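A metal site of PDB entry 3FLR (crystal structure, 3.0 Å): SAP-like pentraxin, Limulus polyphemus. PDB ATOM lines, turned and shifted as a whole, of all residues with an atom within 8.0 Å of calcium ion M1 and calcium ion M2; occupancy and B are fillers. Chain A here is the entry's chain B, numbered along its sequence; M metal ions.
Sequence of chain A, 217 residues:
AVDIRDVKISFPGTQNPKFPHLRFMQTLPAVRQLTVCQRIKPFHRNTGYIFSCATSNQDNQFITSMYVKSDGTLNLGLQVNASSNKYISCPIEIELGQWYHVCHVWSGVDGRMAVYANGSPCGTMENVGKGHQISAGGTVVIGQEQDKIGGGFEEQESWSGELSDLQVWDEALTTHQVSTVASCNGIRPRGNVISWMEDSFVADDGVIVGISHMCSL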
ATOM      1  N   TYR A  49     -25.135 -11.101  33.394  1.00  0.00           N
ATOM      2  CA  TYR A  49     -24.252  -9.977  33.671  1.00  0.00           C
ATOM      3  C   TYR A  49     -24.768  -9.181  34.873  1.00  0.00           C
ATOM      4  O   TYR A  49     -25.953  -8.871  34.965  1.00  0.00           O
ATOM      5  CB  TYR A  49     -24.158  -9.082  32.443  1.00  0.00           C
ATOM      6  CG  TYR A  49     -23.560  -9.763  31.224  1.00  0.00           C
ATOM      7  CD1 TYR A  49     -24.329 -10.601  30.416  1.00  0.00           C
ATOM      8  CD2 TYR A  49     -22.206  -9.604  30.911  1.00  0.00           C
ATOM      9  CE1 TYR A  49     -23.764 -11.250  29.325  1.00  0.00           C
ATOM     10  CE2 TYR A  49     -21.636 -10.253  29.829  1.00  0.00           C
ATOM     11  CZ  TYR A  49     -22.411 -11.074  29.034  1.00  0.00           C
ATOM     12  OH  TYR A  49     -21.837 -11.722  27.961  1.00  0.00           O
ATOM     13  N   SER A  52     -22.762  -3.462  34.689  1.00  0.00           N
ATOM     14  CA  SER A  52     -22.595  -3.036  33.307  1.00  0.00           C
ATOM     15  C   SER A  52     -22.285  -1.543  33.216  1.00  0.00           C
ATOM     16  O   SER A  52     -23.088  -0.710  33.627  1.00  0.00           O
ATOM     17  CB  SER A  52     -23.862  -3.343  32.521  1.00  0.00           C
ATOM     18  OG  SER A  52     -23.715  -3.014  31.144  1.00  0.00           O
ATOM     19  N   CYS A  53     -21.115  -1.199  32.681  1.00  0.00           N
ATOM     20  CA  CYS A  53     -20.713   0.206  32.537  1.00  0.00           C
ATOM     21  C   CYS A  53     -20.633   0.545  31.059  1.00  0.00           C
ATOM     22  O   CYS A  53     -19.875  -0.076  30.317  1.00  0.00           O
ATOM     23  CB  CYS A  53     -19.351   0.463  33.185  1.00  0.00           C
ATOM     24  SG  CYS A  53     -18.831   2.191  33.093  1.00  0.00           S
ATOM     25  N   ALA A  54     -21.418   1.540  30.636  1.00  0.00           N
ATOM     26  CA  ALA A  54     -21.466   1.925  29.233  1.00  0.00           C
ATOM     27  C   ALA A  54     -21.339   3.417  28.989  1.00  0.00           C
ATOM     28  O   ALA A  54     -21.897   4.236  29.714  1.00  0.00           O
ATOM     29  CB  ALA A  54     -22.760   1.420  28.644  1.00  0.00           C
ATOM     30  N   GLN A  58     -19.384   3.154  23.604  1.00  0.00           N
ATOM     31  CA  GLN A  58     -18.870   1.839  23.975  1.00  0.00           C
ATOM     32  C   GLN A  58     -19.754   1.315  25.107  1.00  0.00           C
ATOM     33  O   GLN A  58     -19.508   1.575  26.284  1.00  0.00           O
ATOM     34  CB  GLN A  58     -17.416   1.929  24.417  1.00  0.00           C
ATOM     35  CG  GLN A  58     -16.832   0.637  24.965  1.00  0.00           C
ATOM     36  CD  GLN A  58     -16.821  -0.518  23.972  1.00  0.00           C
ATOM     37  OE1 GLN A  58     -17.874  -1.006  23.561  1.00  0.00           O
ATOM     38  NE2 GLN A  58     -15.621  -0.961  23.587  1.00  0.00           N
ATOM     39  N   ASP A  59     -20.802   0.585  24.720  1.00  0.00           N
ATOM     40  CA  ASP A  59     -21.742   0.022  25.680  1.00  0.00           C
ATOM     41  C   ASP A  59     -21.111  -1.156  26.410  1.00  0.00           C
ATOM     42  O   ASP A  59     -21.694  -1.712  27.352  1.00  0.00           O
ATOM     43  CB  ASP A  59     -23.019  -0.418  24.965  1.00  0.00           C
ATOM     44  CG  ASP A  59     -22.747  -1.439  23.883  1.00  0.00           C
ATOM     45  OD1 ASP A  59     -21.847  -1.207  23.045  1.00  0.00           O
ATOM     46  OD2 ASP A  59     -23.446  -2.482  23.865  1.00  0.00           O
ATOM     47  N   ASN A  60     -19.912  -1.517  25.986  1.00  0.00           N
ATOM     48  CA  ASN A  60     -19.192  -2.611  26.597  1.00  0.00           C
ATOM     49  C   ASN A  60     -17.886  -2.154  27.217  1.00  0.00           C
ATOM     50  O   ASN A  60     -16.835  -2.747  26.976  1.00  0.00           O
ATOM     51  CB  ASN A  60     -18.930  -3.697  25.558  1.00  0.00           C
ATOM     52  CG  ASN A  60     -20.110  -4.626  25.401  1.00  0.00           C
ATOM     53  OD1 ASN A  60     -21.260  -4.185  25.297  1.00  0.00           O
ATOM     54  ND2 ASN A  60     -19.842  -5.931  25.381  1.00  0.00           N
ATOM     55  N   GLN A  61     -17.954  -1.105  28.020  1.00  0.00           N
ATOM     56  CA  GLN A  61     -16.771  -0.573  28.666  1.00  0.00           C
ATOM     57  C   GLN A  61     -16.273  -1.486  29.777  1.00  0.00           C
ATOM     58  O   GLN A  61     -15.081  -1.754  29.871  1.00  0.00           O
ATOM     59  CB  GLN A  61     -17.059   0.817  29.246  1.00  0.00           C
ATOM     60  CG  GLN A  61     -16.954   1.938  28.235  1.00  0.00           C
ATOM     61  CD  GLN A  61     -15.512   2.321  27.962  1.00  0.00           C
ATOM     62  OE1 GLN A  61     -14.605   1.501  28.084  1.00  0.00           O
ATOM     63  NE2 GLN A  61     -15.306   3.576  27.568  1.00  0.00           N
ATOM     64  N   ILE A  63     -17.936  -4.978  32.111  1.00  0.00           N
ATOM     65  CA  ILE A  63     -19.089  -5.810  32.443  1.00  0.00           C
ATOM     66  C   ILE A  63     -18.729  -7.060  33.230  1.00  0.00           C
ATOM     67  O   ILE A  63     -18.041  -7.947  32.712  1.00  0.00           O
ATOM     68  CB  ILE A  63     -19.811  -6.289  31.179  1.00  0.00           C
ATOM     69  CG1 ILE A  63     -19.542  -5.340  30.014  1.00  0.00           C
ATOM     70  CG2 ILE A  63     -21.291  -6.410  31.465  1.00  0.00           C
ATOM     71  CD1 ILE A  63     -20.190  -5.741  28.718  1.00  0.00           C
ATOM     72  N   GLN A  79     -15.288  -8.414  31.186  1.00  0.00           N
ATOM     73  CA  GLN A  79     -15.090  -8.006  29.812  1.00  0.00           C
ATOM     74  C   GLN A  79     -14.755  -6.515  29.832  1.00  0.00           C
ATOM     75  O   GLN A  79     -15.442  -5.731  30.480  1.00  0.00           O
ATOM     76  CB  GLN A  79     -16.349  -8.263  28.984  1.00  0.00           C
ATOM     77  CG  GLN A  79     -16.232  -7.838  27.538  1.00  0.00           C
ATOM     78  CD  GLN A  79     -17.499  -8.118  26.739  1.00  0.00           C
ATOM     79  OE1 GLN A  79     -17.719  -7.540  25.674  1.00  0.00           O
ATOM     80  NE2 GLN A  79     -18.336  -9.023  27.260  1.00  0.00           N
ATOM     81  N   ALA A  82     -15.222  -3.930  25.020  1.00  0.00           N
ATOM     82  CA  ALA A  82     -15.764  -4.832  24.018  1.00  0.00           C
ATOM     83  C   ALA A  82     -14.953  -6.092  23.755  1.00  0.00           C
ATOM     84  O   ALA A  82     -15.156  -6.761  22.740  1.00  0.00           O
ATOM     85  CB  ALA A  82     -15.999  -4.079  22.701  1.00  0.00           C
ATOM     86  N   GLN A 144     -28.655  -6.119  34.346  1.00  0.00           N
ATOM     87  CA  GLN A 144     -28.973  -6.049  32.925  1.00  0.00           C
ATOM     88  C   GLN A 144     -27.713  -5.648  32.192  1.00  0.00           C
ATOM     89  O   GLN A 144     -26.862  -4.961  32.753  1.00  0.00           O
ATOM     90  CB  GLN A 144     -30.056  -5.016  32.633  1.00  0.00           C
ATOM     91  CG  GLN A 144     -31.440  -5.392  33.112  1.00  0.00           C
ATOM     92  CD  GLN A 144     -31.873  -6.769  32.638  1.00  0.00           C
ATOM     93  OE1 GLN A 144     -31.458  -7.230  31.580  1.00  0.00           O
ATOM     94  NE2 GLN A 144     -32.723  -7.413  33.431  1.00  0.00           N
ATOM     95  N   GLU A 145     -27.607  -6.055  30.931  1.00  0.00           N
ATOM     96  CA  GLU A 145     -26.442  -5.734  30.095  1.00  0.00           C
ATOM     97  C   GLU A 145     -26.869  -4.691  29.063  1.00  0.00           C
ATOM     98  O   GLU A 145     -27.697  -4.959  28.180  1.00  0.00           O
ATOM     99  CB  GLU A 145     -25.948  -7.021  29.412  1.00  0.00           C
ATOM    100  CG  GLU A 145     -24.506  -6.985  28.948  1.00  0.00           C
ATOM    101  CD  GLU A 145     -24.284  -6.060  27.764  1.00  0.00           C
ATOM    102  OE1 GLU A 145     -24.878  -6.329  26.690  1.00  0.00           O
ATOM    103  OE2 GLU A 145     -23.520  -5.081  27.909  1.00  0.00           O
ATOM    104  N   GLN A 146     -26.302  -3.485  29.161  1.00  0.00           N
ATOM    105  CA  GLN A 146     -26.653  -2.401  28.245  1.00  0.00           C
ATOM    106  C   GLN A 146     -26.042  -2.539  26.848  1.00  0.00           C
ATOM    107  O   GLN A 146     -24.913  -2.987  26.692  1.00  0.00           O
ATOM    108  CB  GLN A 146     -26.177  -1.055  28.800  1.00  0.00           C
ATOM    109  CG  GLN A 146     -26.398  -0.822  30.281  1.00  0.00           C
ATOM    110  CD  GLN A 146     -25.676   0.430  30.758  1.00  0.00           C
ATOM    111  OE1 GLN A 146     -25.980   1.537  30.336  1.00  0.00           O
ATOM    112  NE2 GLN A 146     -24.702   0.248  31.640  1.00  0.00           N
ATOM    113  N   ASP A 147     -26.816  -2.155  25.837  1.00  0.00           N
ATOM    114  CA  ASP A 147     -26.359  -2.159  24.444  1.00  0.00           C
ATOM    115  C   ASP A 147     -26.609  -0.725  23.994  1.00  0.00           C
ATOM    116  O   ASP A 147     -26.204  -0.291  22.917  1.00  0.00           O
ATOM    117  CB  ASP A 147     -27.158  -3.163  23.606  1.00  0.00           C
ATOM    118  CG  ASP A 147     -26.909  -4.602  24.022  1.00  0.00           C
ATOM    119  OD1 ASP A 147     -25.742  -4.902  24.369  1.00  0.00           O
ATOM    120  OD2 ASP A 147     -27.846  -5.432  24.014  1.00  0.00           O
ATOM    121  N   LYS A 148     -27.239   0.016  24.898  1.00  0.00           N
ATOM    122  CA  LYS A 148     -27.594   1.413  24.721  1.00  0.00           C
ATOM    123  C   LYS A 148     -27.377   2.006  26.118  1.00  0.00           C
ATOM    124  O   LYS A 148     -27.443   1.282  27.116  1.00  0.00           O
ATOM    125  CB  LYS A 148     -29.057   1.494  24.295  1.00  0.00           C
ATOM    126  CG  LYS A 148     -29.527   2.868  23.886  1.00  0.00           C
ATOM    127  CD  LYS A 148     -30.813   2.820  23.070  1.00  0.00           C
ATOM    128  CE  LYS A 148     -32.035   2.429  23.906  1.00  0.00           C
ATOM    129  NZ  LYS A 148     -33.313   2.643  23.160  1.00  0.00           N
ATOM    130  N   GLY A 151     -30.041   1.166  28.531  1.00  0.00           N
ATOM    131  CA  GLY A 151     -31.067   0.457  27.781  1.00  0.00           C
ATOM    132  C   GLY A 151     -30.573  -0.599  26.800  1.00  0.00           C
ATOM    133  O   GLY A 151     -29.389  -0.955  26.790  1.00  0.00           O
ATOM    134  N   GLY A 152     -31.480  -1.094  25.962  1.00  0.00           N
ATOM    135  CA  GLY A 152     -31.102  -2.107  25.005  1.00  0.00           C
ATOM    136  C   GLY A 152     -30.786  -3.403  25.727  1.00  0.00           C
ATOM    137  O   GLY A 152     -29.719  -3.989  25.546  1.00  0.00           O
ATOM    138  N   PHE A 153     -31.709  -3.841  26.568  1.00  0.00           N
ATOM    139  CA  PHE A 153     -31.485  -5.072  27.335  1.00  0.00           C
ATOM    140  C   PHE A 153     -31.912  -6.325  26.578  1.00  0.00           C
ATOM    141  O   PHE A 153     -32.885  -6.306  25.820  1.00  0.00           O
ATOM    142  CB  PHE A 153     -32.228  -5.014  28.682  1.00  0.00           C
ATOM    143  CG  PHE A 153     -31.904  -3.792  29.506  1.00  0.00           C
ATOM    144  CD1 PHE A 153     -30.603  -3.312  29.596  1.00  0.00           C
ATOM    145  CD2 PHE A 153     -32.910  -3.150  30.229  1.00  0.00           C
ATOM    146  CE1 PHE A 153     -30.317  -2.199  30.379  1.00  0.00           C
ATOM    147  CE2 PHE A 153     -32.623  -2.036  31.012  1.00  0.00           C
ATOM    148  CZ  PHE A 153     -31.332  -1.557  31.084  1.00  0.00           C
ATOM    149  N   GLU A 154     -31.161  -7.400  26.764  1.00  0.00           N
ATOM    150  CA  GLU A 154     -31.464  -8.683  26.136  1.00  0.00           C
ATOM    151  C   GLU A 154     -31.752  -9.661  27.279  1.00  0.00           C
ATOM    152  O   GLU A 154     -30.864  -9.958  28.077  1.00  0.00           O
ATOM    153  CB  GLU A 154     -30.287  -9.181  25.303  1.00  0.00           C
ATOM    154  CG  GLU A 154     -29.818  -8.188  24.256  1.00  0.00           C
ATOM    155  CD  GLU A 154     -28.924  -8.804  23.206  1.00  0.00           C
ATOM    156  OE1 GLU A 154     -27.865  -9.375  23.559  1.00  0.00           O
ATOM    157  OE2 GLU A 154     -29.266  -8.720  22.000  1.00  0.00           O
ATOM    158  N   GLU A 155     -32.988 -10.143  27.348  1.00  0.00           N
ATOM    159  CA  GLU A 155     -33.345 -11.031  28.442  1.00  0.00           C
ATOM    160  C   GLU A 155     -32.448 -12.245  28.628  1.00  0.00           C
ATOM    161  O   GLU A 155     -32.386 -12.795  29.718  1.00  0.00           O
ATOM    162  CB  GLU A 155     -34.809 -11.465  28.345  1.00  0.00           C
ATOM    163  CG  GLU A 155     -35.171 -12.393  27.216  1.00  0.00           C
ATOM    164  CD  GLU A 155     -36.681 -12.486  27.030  1.00  0.00           C
ATOM    165  OE1 GLU A 155     -37.273 -11.497  26.528  1.00  0.00           O
ATOM    166  OE2 GLU A 155     -37.277 -13.516  27.399  1.00  0.00           O
ATOM    167  N   GLN A 156     -31.740 -12.664  27.584  1.00  0.00           N
ATOM    168  CA  GLN A 156     -30.861 -13.822  27.741  1.00  0.00           C
ATOM    169  C   GLN A 156     -29.531 -13.425  28.420  1.00  0.00           C
ATOM    170  O   GLN A 156     -28.770 -14.292  28.848  1.00  0.00           O
ATOM    171  CB  GLN A 156     -30.582 -14.495  26.384  1.00  0.00           C
ATOM    172  CG  GLN A 156     -29.507 -13.816  25.527  1.00  0.00           C
ATOM    173  CD  GLN A 156     -30.057 -12.704  24.634  1.00  0.00           C
ATOM    174  OE1 GLN A 156     -30.955 -11.956  25.010  1.00  0.00           O
ATOM    175  NE2 GLN A 156     -29.486 -12.603  23.434  1.00  0.00           N
ATOM    176  N   GLU A 157     -29.272 -12.124  28.538  1.00  0.00           N
ATOM    177  CA  GLU A 157     -28.052 -11.638  29.167  1.00  0.00           C
ATOM    178  C   GLU A 157     -28.285 -11.121  30.590  1.00  0.00           C
ATOM    179  O   GLU A 157     -27.332 -10.819  31.304  1.00  0.00           O
ATOM    180  CB  GLU A 157     -27.442 -10.496  28.343  1.00  0.00           C
ATOM    181  CG  GLU A 157     -27.171 -10.849  26.889  1.00  0.00           C
ATOM    182  CD  GLU A 157     -26.480  -9.725  26.136  1.00  0.00           C
ATOM    183  OE1 GLU A 157     -26.960  -8.565  26.221  1.00  0.00           O
ATOM    184  OE2 GLU A 157     -25.471  -9.993  25.455  1.00  0.00           O
ATOM    185  N   SER A 158     -29.545 -11.030  30.985  1.00  0.00           N
ATOM    186  CA  SER A 158     -29.883 -10.545  32.329  1.00  0.00           C
ATOM    187  C   SER A 158     -29.424 -11.521  33.408  1.00  0.00           C
ATOM    188  O   SER A 158     -29.121 -12.689  33.123  1.00  0.00           O
ATOM    189  CB  SER A 158     -31.382 -10.321  32.433  1.00  0.00           C
ATOM    190  OG  SER A 158     -32.079 -11.521  32.188  1.00  0.00           O
HETATM  191 CA    CA M   1     -26.530  -7.107  24.757  1.00  0.00          CA
HETATM  192 CA    CA M   2     -23.583  -4.488  25.313  1.00  0.00          CA
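O of Gly 152 lies close to N of Asp 147 (3.4 Å). O of Ser 52 is in hydrogen-bond range of NE2 of Gln 146, at 2.7 Å. O of Glu 157 is in hydrogen-bond range of N of Tyr 49. The backbone carbonyl oxygen (O) of Asn 60 lies within hydrogen-bond range of the backbone NH (N) of Ala 82 (2.8 Å). N of Asn 60 sits close to OE1 of Gln 58 (3.2 Å). The side-chain amide nitrogen of Asn 60 sits at hydrogen-bond distance from the side-chain amide oxygen of Gln 79 (2.7 Å).
Of the 24 residues printed, 4 come within 4 Å of calcium ion M1. The nearest printed residue that does not touch calcium ion M1 is Gly 152 (4.5 Å).
Calcium ion M1 is bound by OE1 of Glu 157 (2.1 Å), OD2 of Asp 147 (2.3 Å), OD1 of Asp 147 (2.4 Å), OE1 of Glu 145 (2.7 Å) and OE1 of Glu 154 (2.9 Å). Calcium ion M1 has five donor atoms within binding distance.
Calcium ion M2 is bound by the side-chain amide oxygen (OD1) of Asn 60 (2.3 Å), the side-chain carboxylate (OD1) of Asp 147 (2.4 Å), the backbone carbonyl oxygen (O) of Gln 146 (2.4 Å), the side-chain carboxylate (OD2) of Asp 59 (2.5 Å), the side-chain carboxylate (OE1) of Glu 145 (2.6 Å) and the side-chain carboxylate (OE2) of Glu 145 (2.7 Å).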
